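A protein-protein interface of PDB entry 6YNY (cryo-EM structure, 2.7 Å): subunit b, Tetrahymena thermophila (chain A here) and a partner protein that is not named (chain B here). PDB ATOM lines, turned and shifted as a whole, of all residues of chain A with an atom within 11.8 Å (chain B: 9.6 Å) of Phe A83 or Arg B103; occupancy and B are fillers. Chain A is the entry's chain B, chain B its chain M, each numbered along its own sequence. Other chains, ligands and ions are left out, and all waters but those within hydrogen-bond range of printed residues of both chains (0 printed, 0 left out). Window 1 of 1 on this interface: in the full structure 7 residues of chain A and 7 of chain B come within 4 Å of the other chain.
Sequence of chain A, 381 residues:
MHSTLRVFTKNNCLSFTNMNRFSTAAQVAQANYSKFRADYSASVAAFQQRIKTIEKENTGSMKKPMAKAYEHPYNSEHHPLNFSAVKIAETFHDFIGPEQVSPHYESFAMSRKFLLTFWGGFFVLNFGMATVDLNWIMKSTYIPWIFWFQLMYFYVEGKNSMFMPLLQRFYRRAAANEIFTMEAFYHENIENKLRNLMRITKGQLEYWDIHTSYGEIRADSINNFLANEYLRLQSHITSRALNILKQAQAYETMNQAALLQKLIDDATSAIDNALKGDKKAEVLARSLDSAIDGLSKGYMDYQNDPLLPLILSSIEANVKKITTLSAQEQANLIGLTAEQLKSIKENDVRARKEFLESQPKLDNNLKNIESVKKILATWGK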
ATOM      1  N   TYR A  74     -22.452 -30.111  19.271  1.00  0.00           N
ATOM      2  CA  TYR A  74     -21.304 -30.254  18.385  1.00  0.00           C
ATOM      3  C   TYR A  74     -20.315 -29.110  18.555  1.00  0.00           C
ATOM      4  O   TYR A  74     -19.556 -28.796  17.636  1.00  0.00           O
ATOM      5  CB  TYR A  74     -21.751 -30.364  16.928  1.00  0.00           C
ATOM      6  CG  TYR A  74     -22.411 -31.678  16.605  1.00  0.00           C
ATOM      7  CD1 TYR A  74     -21.654 -32.823  16.426  1.00  0.00           C
ATOM      8  CD2 TYR A  74     -23.784 -31.778  16.478  1.00  0.00           C
ATOM      9  CE1 TYR A  74     -22.243 -34.026  16.136  1.00  0.00           C
ATOM     10  CE2 TYR A  74     -24.383 -32.980  16.189  1.00  0.00           C
ATOM     11  CZ  TYR A  74     -23.608 -34.102  16.015  1.00  0.00           C
ATOM     12  OH  TYR A  74     -24.196 -35.309  15.721  1.00  0.00           O
ATOM     13  N   ASN A  75     -20.308 -28.478  19.724  1.00  0.00           N
ATOM     14  CA  ASN A  75     -19.348 -27.428  20.031  1.00  0.00           C
ATOM     15  C   ASN A  75     -18.812 -27.657  21.433  1.00  0.00           C
ATOM     16  O   ASN A  75     -19.589 -27.844  22.373  1.00  0.00           O
ATOM     17  CB  ASN A  75     -19.976 -26.039  19.925  1.00  0.00           C
ATOM     18  CG  ASN A  75     -18.973 -24.932  20.133  1.00  0.00           C
ATOM     19  OD1 ASN A  75     -17.825 -25.031  19.704  1.00  0.00           O
ATOM     20  ND2 ASN A  75     -19.396 -23.874  20.802  1.00  0.00           N
ATOM     21  N   SER A  76     -17.489 -27.652  21.567  1.00  0.00           N
ATOM     22  CA  SER A  76     -16.838 -27.815  22.855  1.00  0.00           C
ATOM     23  C   SER A  76     -15.668 -26.850  22.945  1.00  0.00           C
ATOM     24  O   SER A  76     -15.311 -26.176  21.976  1.00  0.00           O
ATOM     25  CB  SER A  76     -16.361 -29.254  23.068  1.00  0.00           C
ATOM     26  OG  SER A  76     -15.355 -29.605  22.139  1.00  0.00           O
ATOM     27  N   GLU A  77     -15.071 -26.787  24.133  1.00  0.00           N
ATOM     28  CA  GLU A  77     -13.966 -25.865  24.361  1.00  0.00           C
ATOM     29  C   GLU A  77     -12.681 -26.366  23.714  1.00  0.00           C
ATOM     30  O   GLU A  77     -11.892 -25.568  23.197  1.00  0.00           O
ATOM     31  CB  GLU A  77     -13.769 -25.651  25.860  1.00  0.00           C
ATOM     32  CG  GLU A  77     -12.788 -24.550  26.208  1.00  0.00           C
ATOM     33  CD  GLU A  77     -12.745 -24.256  27.695  1.00  0.00           C
ATOM     34  OE1 GLU A  77     -13.326 -25.040  28.473  1.00  0.00           O
ATOM     35  OE2 GLU A  77     -12.137 -23.237  28.085  1.00  0.00           O
ATOM     36  N   HIS A  78     -12.458 -27.678  23.728  1.00  0.00           N
ATOM     37  CA  HIS A  78     -11.264 -28.255  23.125  1.00  0.00           C
ATOM     38  C   HIS A  78     -11.442 -28.537  21.642  1.00  0.00           C
ATOM     39  O   HIS A  78     -10.457 -28.541  20.897  1.00  0.00           O
ATOM     40  CB  HIS A  78     -10.881 -29.544  23.849  1.00  0.00           C
ATOM     41  CG  HIS A  78      -9.580 -30.124  23.398  1.00  0.00           C
ATOM     42  ND1 HIS A  78      -8.407 -29.403  23.392  1.00  0.00           N
ATOM     43  CD2 HIS A  78      -9.266 -31.357  22.938  1.00  0.00           C
ATOM     44  CE1 HIS A  78      -7.427 -30.166  22.947  1.00  0.00           C
ATOM     45  NE2 HIS A  78      -7.921 -31.357  22.666  1.00  0.00           N
ATOM     46  N   HIS A  79     -12.676 -28.772  21.199  1.00  0.00           N
ATOM     47  CA  HIS A  79     -12.999 -28.988  19.793  1.00  0.00           C
ATOM     48  C   HIS A  79     -14.039 -27.959  19.364  1.00  0.00           C
ATOM     49  O   HIS A  79     -15.188 -28.308  19.063  1.00  0.00           O
ATOM     50  CB  HIS A  79     -13.518 -30.401  19.548  1.00  0.00           C
ATOM     51  CG  HIS A  79     -12.488 -31.467  19.731  1.00  0.00           C
ATOM     52  ND1 HIS A  79     -11.679 -31.900  18.703  1.00  0.00           N
ATOM     53  CD2 HIS A  79     -12.144 -32.201  20.814  1.00  0.00           C
ATOM     54  CE1 HIS A  79     -10.876 -32.847  19.149  1.00  0.00           C
ATOM     55  NE2 HIS A  79     -11.137 -33.048  20.426  1.00  0.00           N
ATOM     56  N   PRO A  80     -13.671 -26.681  19.327  1.00  0.00           N
ATOM     57  CA  PRO A  80     -14.630 -25.658  18.910  1.00  0.00           C
ATOM     58  C   PRO A  80     -15.098 -25.880  17.482  1.00  0.00           C
ATOM     59  O   PRO A  80     -14.325 -26.266  16.604  1.00  0.00           O
ATOM     60  CB  PRO A  80     -13.842 -24.353  19.054  1.00  0.00           C
ATOM     61  CG  PRO A  80     -12.430 -24.753  19.117  1.00  0.00           C
ATOM     62  CD  PRO A  80     -12.390 -26.091  19.734  1.00  0.00           C
ATOM     63  N   LEU A  81     -16.387 -25.624  17.258  1.00  0.00           N
ATOM     64  CA  LEU A  81     -16.972 -25.886  15.950  1.00  0.00           C
ATOM     65  C   LEU A  81     -16.445 -24.921  14.900  1.00  0.00           C
ATOM     66  O   LEU A  81     -16.133 -25.328  13.776  1.00  0.00           O
ATOM     67  CB  LEU A  81     -18.491 -25.794  16.042  1.00  0.00           C
ATOM     68  CG  LEU A  81     -19.266 -26.040  14.755  1.00  0.00           C
ATOM     69  CD1 LEU A  81     -18.923 -27.388  14.167  1.00  0.00           C
ATOM     70  CD2 LEU A  81     -20.733 -25.948  15.039  1.00  0.00           C
ATOM     71  N   ASN A  82     -16.340 -23.645  15.244  1.00  0.00           N
ATOM     72  CA  ASN A  82     -15.892 -22.616  14.324  1.00  0.00           C
ATOM     73  C   ASN A  82     -14.415 -22.311  14.534  1.00  0.00           C
ATOM     74  O   ASN A  82     -13.820 -22.659  15.557  1.00  0.00           O
ATOM     75  CB  ASN A  82     -16.738 -21.356  14.490  1.00  0.00           C
ATOM     76  CG  ASN A  82     -18.179 -21.582  14.104  1.00  0.00           C
ATOM     77  OD1 ASN A  82     -18.469 -22.082  13.020  1.00  0.00           O
ATOM     78  ND2 ASN A  82     -19.093 -21.236  14.997  1.00  0.00           N
ATOM     79  N   PHE A  83     -13.827 -21.652  13.544  1.00  0.00           N
ATOM     80  CA  PHE A  83     -12.385 -21.509  13.445  1.00  0.00           C
ATOM     81  C   PHE A  83     -11.950 -20.060  13.616  1.00  0.00           C
ATOM     82  O   PHE A  83     -12.654 -19.125  13.229  1.00  0.00           O
ATOM     83  CB  PHE A  83     -11.887 -22.042  12.104  1.00  0.00           C
ATOM     84  CG  PHE A  83     -12.036 -23.519  11.960  1.00  0.00           C
ATOM     85  CD1 PHE A  83     -11.049 -24.368  12.407  1.00  0.00           C
ATOM     86  CD2 PHE A  83     -13.169 -24.059  11.391  1.00  0.00           C
ATOM     87  CE1 PHE A  83     -11.187 -25.726  12.283  1.00  0.00           C
ATOM     88  CE2 PHE A  83     -13.309 -25.416  11.266  1.00  0.00           C
ATOM     89  CZ  PHE A  83     -12.316 -26.249  11.714  1.00  0.00           C
ATOM     90  N   SER A  84     -10.772 -19.898  14.209  1.00  0.00           N
ATOM     91  CA  SER A  84     -10.143 -18.603  14.410  1.00  0.00           C
ATOM     92  C   SER A  84      -8.687 -18.849  14.772  1.00  0.00           C
ATOM     93  O   SER A  84      -8.311 -19.948  15.188  1.00  0.00           O
ATOM     94  CB  SER A  84     -10.836 -17.796  15.509  1.00  0.00           C
ATOM     95  OG  SER A  84     -10.771 -18.480  16.749  1.00  0.00           O
ATOM     96  N   ALA A  85      -7.873 -17.810  14.607  1.00  0.00           N
ATOM     97  CA  ALA A  85      -6.471 -17.890  14.989  1.00  0.00           C
ATOM     98  C   ALA A  85      -6.276 -17.928  16.496  1.00  0.00           C
ATOM     99  O   ALA A  85      -5.154 -18.166  16.950  1.00  0.00           O
ATOM    100  CB  ALA A  85      -5.703 -16.712  14.398  1.00  0.00           C
ATOM    101  N   VAL A  86      -7.335 -17.712  17.273  1.00  0.00           N
ATOM    102  CA  VAL A  86      -7.210 -17.709  18.726  1.00  0.00           C
ATOM    103  C   VAL A  86      -6.999 -19.123  19.249  1.00  0.00           C
ATOM    104  O   VAL A  86      -6.137 -19.364  20.101  1.00  0.00           O
ATOM    105  CB  VAL A  86      -8.442 -17.045  19.360  1.00  0.00           C
ATOM    106  CG1 VAL A  86      -8.324 -17.020  20.864  1.00  0.00           C
ATOM    107  CG2 VAL A  86      -8.606 -15.644  18.822  1.00  0.00           C
ATOM    108  N   LYS A  87      -7.783 -20.081  18.754  1.00  0.00           N
ATOM    109  CA  LYS A  87      -7.615 -21.456  19.206  1.00  0.00           C
ATOM    110  C   LYS A  87      -6.318 -22.052  18.681  1.00  0.00           C
ATOM    111  O   LYS A  87      -5.665 -22.839  19.372  1.00  0.00           O
ATOM    112  CB  LYS A  87      -8.808 -22.305  18.772  1.00  0.00           C
ATOM    113  CG  LYS A  87      -8.787 -23.723  19.306  1.00  0.00           C
ATOM    114  CD  LYS A  87      -9.028 -23.759  20.793  1.00  0.00           C
ATOM    115  CE  LYS A  87      -8.867 -25.151  21.352  1.00  0.00           C
ATOM    116  NZ  LYS A  87      -9.167 -25.174  22.803  1.00  0.00           N
ATOM    117  N   ILE A  88      -5.932 -21.690  17.458  1.00  0.00           N
ATOM    118  CA  ILE A  88      -4.654 -22.142  16.920  1.00  0.00           C
ATOM    119  C   ILE A  88      -3.508 -21.620  17.773  1.00  0.00           C
ATOM    120  O   ILE A  88      -2.511 -22.317  17.996  1.00  0.00           O
ATOM    121  CB  ILE A  88      -4.515 -21.700  15.451  1.00  0.00           C
ATOM    122  CG1 ILE A  88      -5.647 -22.287  14.614  1.00  0.00           C
ATOM    123  CG2 ILE A  88      -3.182 -22.125  14.889  1.00  0.00           C
ATOM    124  CD1 ILE A  88      -5.696 -21.759  13.211  1.00  0.00           C
ATOM    125  N   ALA A  89      -3.631 -20.388  18.263  1.00  0.00           N
ATOM    126  CA  ALA A  89      -2.608 -19.836  19.140  1.00  0.00           C
ATOM    127  C   ALA A  89      -2.559 -20.580  20.465  1.00  0.00           C
ATOM    128  O   ALA A  89      -1.480 -20.787  21.030  1.00  0.00           O
ATOM    129  CB  ALA A  89      -2.868 -18.353  19.368  1.00  0.00           C
ATOM    130  N   GLU A  90      -3.720 -20.984  20.979  1.00  0.00           N
ATOM    131  CA  GLU A  90      -3.755 -21.747  22.219  1.00  0.00           C
ATOM    132  C   GLU A  90      -3.050 -23.085  22.057  1.00  0.00           C
ATOM    133  O   GLU A  90      -2.307 -23.515  22.946  1.00  0.00           O
ATOM    134  CB  GLU A  90      -5.202 -21.945  22.660  1.00  0.00           C
ATOM    135  CG  GLU A  90      -5.361 -22.465  24.068  1.00  0.00           C
ATOM    136  CD  GLU A  90      -6.777 -22.912  24.368  1.00  0.00           C
ATOM    137  OE1 GLU A  90      -7.186 -23.977  23.865  1.00  0.00           O
ATOM    138  OE2 GLU A  90      -7.484 -22.200  25.110  1.00  0.00           O
ATOM    139  N   THR A  91      -3.268 -23.759  20.925  1.00  0.00           N
ATOM    140  CA  THR A  91      -2.606 -25.035  20.688  1.00  0.00           C
ATOM    141  C   THR A  91      -1.130 -24.850  20.378  1.00  0.00           C
ATOM    142  O   THR A  91      -0.316 -25.716  20.709  1.00  0.00           O
ATOM    143  CB  THR A  91      -3.282 -25.781  19.541  1.00  0.00           C
ATOM    144  OG1 THR A  91      -3.153 -25.029  18.332  1.00  0.00           O
ATOM    145  CG2 THR A  91      -4.736 -25.998  19.835  1.00  0.00           C
ATOM    146  N   ASN B  94     -11.922 -35.097  14.626  1.00  0.00           N
ATOM    147  CA  ASN B  94     -12.527 -33.847  14.189  1.00  0.00           C
ATOM    148  C   ASN B  94     -13.955 -34.068  13.702  1.00  0.00           C
ATOM    149  O   ASN B  94     -14.414 -33.418  12.763  1.00  0.00           O
ATOM    150  CB  ASN B  94     -11.701 -33.201  13.084  1.00  0.00           C
ATOM    151  CG  ASN B  94     -10.238 -33.086  13.427  1.00  0.00           C
ATOM    152  OD1 ASN B  94      -9.393 -33.736  12.818  1.00  0.00           O
ATOM    153  ND2 ASN B  94      -9.926 -32.241  14.393  1.00  0.00           N
ATOM    154  N   TYR B  95     -14.682 -34.979  14.348  1.00  0.00           N
ATOM    155  CA  TYR B  95     -16.002 -35.359  13.854  1.00  0.00           C
ATOM    156  C   TYR B  95     -16.978 -34.192  13.911  1.00  0.00           C
ATOM    157  O   TYR B  95     -17.725 -33.947  12.958  1.00  0.00           O
ATOM    158  CB  TYR B  95     -16.538 -36.541  14.659  1.00  0.00           C
ATOM    159  CG  TYR B  95     -17.903 -37.000  14.216  1.00  0.00           C
ATOM    160  CD1 TYR B  95     -18.054 -37.806  13.103  1.00  0.00           C
ATOM    161  CD2 TYR B  95     -19.039 -36.622  14.907  1.00  0.00           C
ATOM    162  CE1 TYR B  95     -19.291 -38.221  12.693  1.00  0.00           C
ATOM    163  CE2 TYR B  95     -20.282 -37.033  14.503  1.00  0.00           C
ATOM    164  CZ  TYR B  95     -20.404 -37.833  13.395  1.00  0.00           C
ATOM    165  OH  TYR B  95     -21.646 -38.248  12.986  1.00  0.00           O
ATOM    166  N   ASN B  96     -16.994 -33.463  15.024  1.00  0.00           N
ATOM    167  CA  ASN B  96     -17.968 -32.393  15.183  1.00  0.00           C
ATOM    168  C   ASN B  96     -17.782 -31.300  14.142  1.00  0.00           C
ATOM    169  O   ASN B  96     -18.760 -30.686  13.707  1.00  0.00           O
ATOM    170  CB  ASN B  96     -17.871 -31.806  16.586  1.00  0.00           C
ATOM    171  CG  ASN B  96     -16.523 -31.191  16.867  1.00  0.00           C
ATOM    172  OD1 ASN B  96     -15.485 -31.761  16.538  1.00  0.00           O
ATOM    173  ND2 ASN B  96     -16.533 -30.016  17.472  1.00  0.00           N
ATOM    174  N   ASN B  97     -16.544 -31.047  13.729  1.00  0.00           N
ATOM    175  CA  ASN B  97     -16.286 -30.004  12.748  1.00  0.00           C
ATOM    176  C   ASN B  97     -16.667 -30.455  11.343  1.00  0.00           C
ATOM    177  O   ASN B  97     -17.341 -29.724  10.610  1.00  0.00           O
ATOM    178  CB  ASN B  97     -14.815 -29.604  12.797  1.00  0.00           C
ATOM    179  CG  ASN B  97     -14.409 -29.017  14.123  1.00  0.00           C
ATOM    180  OD1 ASN B  97     -13.955 -29.727  15.018  1.00  0.00           O
ATOM    181  ND2 ASN B  97     -14.557 -27.713  14.257  1.00  0.00           N
ATOM    182  N   PHE B  98     -16.242 -31.656  10.952  1.00  0.00           N
ATOM    183  CA  PHE B  98     -16.577 -32.172   9.630  1.00  0.00           C
ATOM    184  C   PHE B  98     -18.073 -32.384   9.459  1.00  0.00           C
ATOM    185  O   PHE B  98     -18.590 -32.288   8.341  1.00  0.00           O
ATOM    186  CB  PHE B  98     -15.844 -33.488   9.380  1.00  0.00           C
ATOM    187  CG  PHE B  98     -14.386 -33.331   9.095  1.00  0.00           C
ATOM    188  CD1 PHE B  98     -13.938 -32.409   8.174  1.00  0.00           C
ATOM    189  CD2 PHE B  98     -13.462 -34.115   9.746  1.00  0.00           C
ATOM    190  CE1 PHE B  98     -12.601 -32.273   7.916  1.00  0.00           C
ATOM    191  CE2 PHE B  98     -12.123 -33.980   9.489  1.00  0.00           C
ATOM    192  CZ  PHE B  98     -11.693 -33.059   8.572  1.00  0.00           C
ATOM    193  N   THR B  99     -18.784 -32.666  10.545  1.00  0.00           N
ATOM    194  CA  THR B  99     -20.195 -33.019  10.465  1.00  0.00           C
ATOM    195  C   THR B  99     -21.121 -31.815  10.575  1.00  0.00           C
ATOM    196  O   THR B  99     -22.135 -31.755   9.874  1.00  0.00           O
ATOM    197  CB  THR B  99     -20.535 -34.031  11.560  1.00  0.00           C
ATOM    198  OG1 THR B  99     -19.662 -35.160  11.454  1.00  0.00           O
ATOM    199  CG2 THR B  99     -21.953 -34.496  11.434  1.00  0.00           C
ATOM    200  N   ALA B 100     -20.801 -30.854  11.436  1.00  0.00           N
ATOM    201  CA  ALA B 100     -21.696 -29.734  11.694  1.00  0.00           C
ATOM    202  C   ALA B 100     -21.311 -28.461  10.961  1.00  0.00           C
ATOM    203  O   ALA B 100     -22.187 -27.641  10.675  1.00  0.00           O
ATOM    204  CB  ALA B 100     -21.753 -29.448  13.194  1.00  0.00           C
ATOM    205  N   ASN B 101     -20.034 -28.265  10.656  1.00  0.00           N
ATOM    206  CA  ASN B 101     -19.600 -27.074   9.939  1.00  0.00           C
ATOM    207  C   ASN B 101     -19.784 -27.292   8.444  1.00  0.00           C
ATOM    208  O   ASN B 101     -19.213 -28.224   7.870  1.00  0.00           O
ATOM    209  CB  ASN B 101     -18.145 -26.756  10.266  1.00  0.00           C
ATOM    210  CG  ASN B 101     -17.736 -25.379   9.808  1.00  0.00           C
ATOM    211  OD1 ASN B 101     -18.134 -24.921   8.739  1.00  0.00           O
ATOM    212  ND2 ASN B 101     -16.941 -24.706  10.620  1.00  0.00           N
ATOM    213  N   ILE B 102     -20.580 -26.427   7.812  1.00  0.00           N
ATOM    214  CA  ILE B 102     -20.883 -26.593   6.398  1.00  0.00           C
ATOM    215  C   ILE B 102     -19.690 -26.261   5.520  1.00  0.00           C
ATOM    216  O   ILE B 102     -19.641 -26.687   4.362  1.00  0.00           O
ATOM    217  CB  ILE B 102     -22.099 -25.737   6.009  1.00  0.00           C
ATOM    218  CG1 ILE B 102     -21.792 -24.248   6.164  1.00  0.00           C
ATOM    219  CG2 ILE B 102     -23.276 -26.107   6.865  1.00  0.00           C
ATOM    220  CD1 ILE B 102     -22.954 -23.362   5.846  1.00  0.00           C
ATOM    221  N   ARG B 103     -18.721 -25.510   6.037  1.00  0.00           N
ATOM    222  CA  ARG B 103     -17.525 -25.219   5.264  1.00  0.00           C
ATOM    223  C   ARG B 103     -16.685 -26.458   5.001  1.00  0.00           C
ATOM    224  O   ARG B 103     -15.779 -26.405   4.164  1.00  0.00           O
ATOM    225  CB  ARG B 103     -16.680 -24.172   5.979  1.00  0.00           C
ATOM    226  CG  ARG B 103     -17.327 -22.806   6.088  1.00  0.00           C
ATOM    227  CD  ARG B 103     -16.276 -21.729   6.165  1.00  0.00           C
ATOM    228  NE  ARG B 103     -15.498 -21.795   7.394  1.00  0.00           N
ATOM    229  CZ  ARG B 103     -14.228 -21.422   7.499  1.00  0.00           C
ATOM    230  NH1 ARG B 103     -13.570 -20.966   6.444  1.00  0.00           N
ATOM    231  NH2 ARG B 103     -13.606 -21.517   8.660  1.00  0.00           N
ATOM    232  N   LEU B 104     -16.961 -27.563   5.693  1.00  0.00           N
ATOM    233  CA  LEU B 104     -16.258 -28.821   5.497  1.00  0.00           C
ATOM    234  C   LEU B 104     -17.163 -29.894   4.907  1.00  0.00           C
ATOM    235  O   LEU B 104     -16.845 -31.083   4.988  1.00  0.00           O
ATOM    236  CB  LEU B 104     -15.671 -29.293   6.823  1.00  0.00           C
ATOM    237  CG  LEU B 104     -14.654 -28.346   7.450  1.00  0.00           C
ATOM    238  CD1 LEU B 104     -14.397 -28.712   8.884  1.00  0.00           C
ATOM    239  CD2 LEU B 104     -13.371 -28.371   6.663  1.00  0.00           C
ATOM    240  N   ARG B 105     -18.282 -29.493   4.305  1.00  0.00           N
ATOM    241  CA  ARG B 105     -19.235 -30.459   3.775  1.00  0.00           C
ATOM    242  C   ARG B 105     -18.608 -31.326   2.694  1.00  0.00           C
ATOM    243  O   ARG B 105     -18.864 -32.532   2.627  1.00  0.00           O
ATOM    244  CB  ARG B 105     -20.459 -29.726   3.231  1.00  0.00           C
ATOM    245  CG  ARG B 105     -20.155 -28.839   2.049  1.00  0.00           C
ATOM    246  CD  ARG B 105     -21.320 -27.952   1.666  1.00  0.00           C
ATOM    247  NE  ARG B 105     -20.969 -27.075   0.558  1.00  0.00           N
ATOM    248  CZ  ARG B 105     -20.264 -25.958   0.690  1.00  0.00           C
ATOM    249  NH1 ARG B 105     -19.830 -25.580   1.879  1.00  0.00           N
ATOM    250  NH2 ARG B 105     -19.984 -25.218  -0.370  1.00  0.00           N
ATOM    251  N   THR B 106     -17.780 -30.730   1.835  1.00  0.00           N
ATOM    252  CA  THR B 106     -17.190 -31.483   0.736  1.00  0.00           C
ATOM    253  C   THR B 106     -16.337 -32.631   1.255  1.00  0.00           C
ATOM    254  O   THR B 106     -16.283 -33.702   0.640  1.00  0.00           O
ATOM    255  CB  THR B 106     -16.368 -30.552  -0.149  1.00  0.00           C
ATOM    256  OG1 THR B 106     -17.222 -29.553  -0.715  1.00  0.00           O
ATOM    257  CG2 THR B 106     -15.699 -31.321  -1.262  1.00  0.00           C
ATOM    258  N   MET B 107     -15.661 -32.430   2.385  1.00  0.00           N
ATOM    259  CA  MET B 107     -14.906 -33.517   2.991  1.00  0.00           C
ATOM    260  C   MET B 107     -15.841 -34.561   3.582  1.00  0.00           C
ATOM    261  O   MET B 107     -15.624 -35.764   3.411  1.00  0.00           O
ATOM    262  CB  MET B 107     -13.964 -32.967   4.059  1.00  0.00           C
ATOM    263  CG  MET B 107     -13.142 -34.020   4.770  1.00  0.00           C
ATOM    264  SD  MET B 107     -12.052 -34.940   3.674  1.00  0.00           S
ATOM    265  CE  MET B 107     -10.744 -33.746   3.455  1.00  0.00           C
ATOM    266  N   ARG B 108     -16.892 -34.120   4.273  1.00  0.00           N
ATOM    267  CA  ARG B 108     -17.856 -35.060   4.825  1.00  0.00           C
ATOM    268  C   ARG B 108     -18.481 -35.917   3.737  1.00  0.00           C
ATOM    269  O   ARG B 108     -18.772 -37.096   3.966  1.00  0.00           O
ATOM    270  CB  ARG B 108     -18.938 -34.302   5.587  1.00  0.00           C
ATOM    271  CG  ARG B 108     -19.992 -35.182   6.223  1.00  0.00           C
ATOM    272  CD  ARG B 108     -21.152 -34.374   6.740  1.00  0.00           C
ATOM    273  NE  ARG B 108     -22.124 -35.203   7.440  1.00  0.00           N
ATOM    274  CZ  ARG B 108     -23.339 -34.797   7.782  1.00  0.00           C
ATOM    275  NH1 ARG B 108     -23.742 -33.573   7.487  1.00  0.00           N
ATOM    276  NH2 ARG B 108     -24.152 -35.620   8.418  1.00  0.00           N
ATOM    277  N   TYR B 109     -18.693 -35.349   2.552  1.00  0.00           N
ATOM    278  CA  TYR B 109     -19.387 -36.067   1.492  1.00  0.00           C
ATOM    279  C   TYR B 109     -18.450 -36.994   0.731  1.00  0.00           C
ATOM    280  O   TYR B 109     -18.842 -38.107   0.363  1.00  0.00           O
ATOM    281  CB  TYR B 109     -20.037 -35.087   0.517  1.00  0.00           C
ATOM    282  CG  TYR B 109     -21.077 -34.160   1.105  1.00  0.00           C
ATOM    283  CD1 TYR B 109     -21.634 -33.155   0.336  1.00  0.00           C
ATOM    284  CD2 TYR B 109     -21.503 -34.286   2.415  1.00  0.00           C
ATOM    285  CE1 TYR B 109     -22.579 -32.305   0.849  1.00  0.00           C
ATOM    286  CE2 TYR B 109     -22.447 -33.435   2.938  1.00  0.00           C
ATOM    287  CZ  TYR B 109     -22.984 -32.448   2.150  1.00  0.00           C
ATOM    288  OH  TYR B 109     -23.931 -31.595   2.661  1.00  0.00           O
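Phe A83 touches just these residues of chain B: Asn B97, Asn B101 and Arg B103.
Arg B103 touches one residue of chain A.
Ser A84 touches none of the printed residues of chain B.
Asn B97 touches just these residues of chain A: Pro A80 (2.8 Å), Leu A81 (2.9 Å) and Phe A83 (3.7 Å).
Of chain A, only Leu A81 (3.3 Å), Asn A82 (3.9 Å) and Phe A83 (3.8 Å) come within 4 Å of Asn B101.
No residue of chain A comes within 4 Å of Leu B104.
No residue of chain A comes within 4 Å of Arg B105.
Printed residues of chain B within 4 Å of Pro A80: Asn B97.
Printed residues of chain A within 4 Å of Ala B100: Tyr A74 and Leu A81.
The nearest residue of chain B that does not touch Phe A83 is Leu B104 (4.2 Å).
The nearest printed residue of chain A that does not touch Tyr B95 is His A79 (6.1 Å).
Tyr A74 touches Tyr B95 (CE1 to CE2, 3.9 Å).
Tyr A74 touches Ala B100 (CB to CB, 3.8 Å).
Leu A81 touches Asn B96 (CD1 to O, 3.3 Å).
Leu A81 touches Ala B100 (CD1 to CB, 3.6 Å).
OD1 of Asn A82 touches ND2 of Asn B101, 3.9 Å away.
Asn B97 touches Phe A83.
Phe A83 touches Asn B101 (CE2 to ND2, 3.8 Å).
Arg B103 touches Phe A83 (NH2 to CD2, 3.8 Å).
ND2 of Asn B96 lies within hydrogen-bond range of O of Tyr A74 (3.3 Å).
O of His A79 lies within hydrogen-bond range of ND2 of Asn B96, at 2.7 Å.
The backbone carbonyl oxygen of Pro A80 is in hydrogen-bond range of the side-chain amide nitrogen of Asn B97.
ND2 of Asn B97 sits at hydrogen-bond distance from O of Leu A81 (2.9 Å).
The side-chain amide nitrogen (ND2) of Asn B101 sits at hydrogen-bond distance from the backbone carbonyl oxygen (O) of Leu A81 (3.3 Å).
The side-chain hydroxyl (OG1) of Thr B99 sits at hydrogen-bond distance from the backbone carbonyl oxygen (O) of Tyr B95 (2.7 Å).
The side-chain amide oxygen (OD1) of Asn B96 sits close to the side-chain amide oxygen (OD1) of Asn B97 (3.0 Å).
The side-chain amide oxygen of Asn B101 sits at hydrogen-bond distance from the backbone NH of Arg B103, 2.8 Å away.
The backbone NH (N) of Leu A81 sits at hydrogen-bond distance from the side-chain amide oxygen (OD1) of Asn A75 (2.9 Å).
The backbone NH (N) of His A79 sits at hydrogen-bond distance from the side-chain hydroxyl (OG) of Ser A76.
Of the 16 printed residues of chain B, 6 touch a printed residue of chain A.
Printed residues of chain B that touch a printed residue of chain A: Tyr B95, Asn B96, Asn B97, Ala B100, Asn B101 and Arg B103.
Printed residues of chain A that touch a printed residue of chain B: Tyr A74, His A79, Pro A80, Leu A81, Asn A82 and Phe A83.
Hydrophobic or aromatic side chains of chain A that line the printed part of chain B: Tyr A74, His A79, Leu A81 and Phe A83.
Among the printed residues, 13 pairs touch across the chains.
Among the printed residues, no Asp or Glu carboxylate lies within 4 Å of a Lys or Arg side-chain nitrogen of the other chain.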
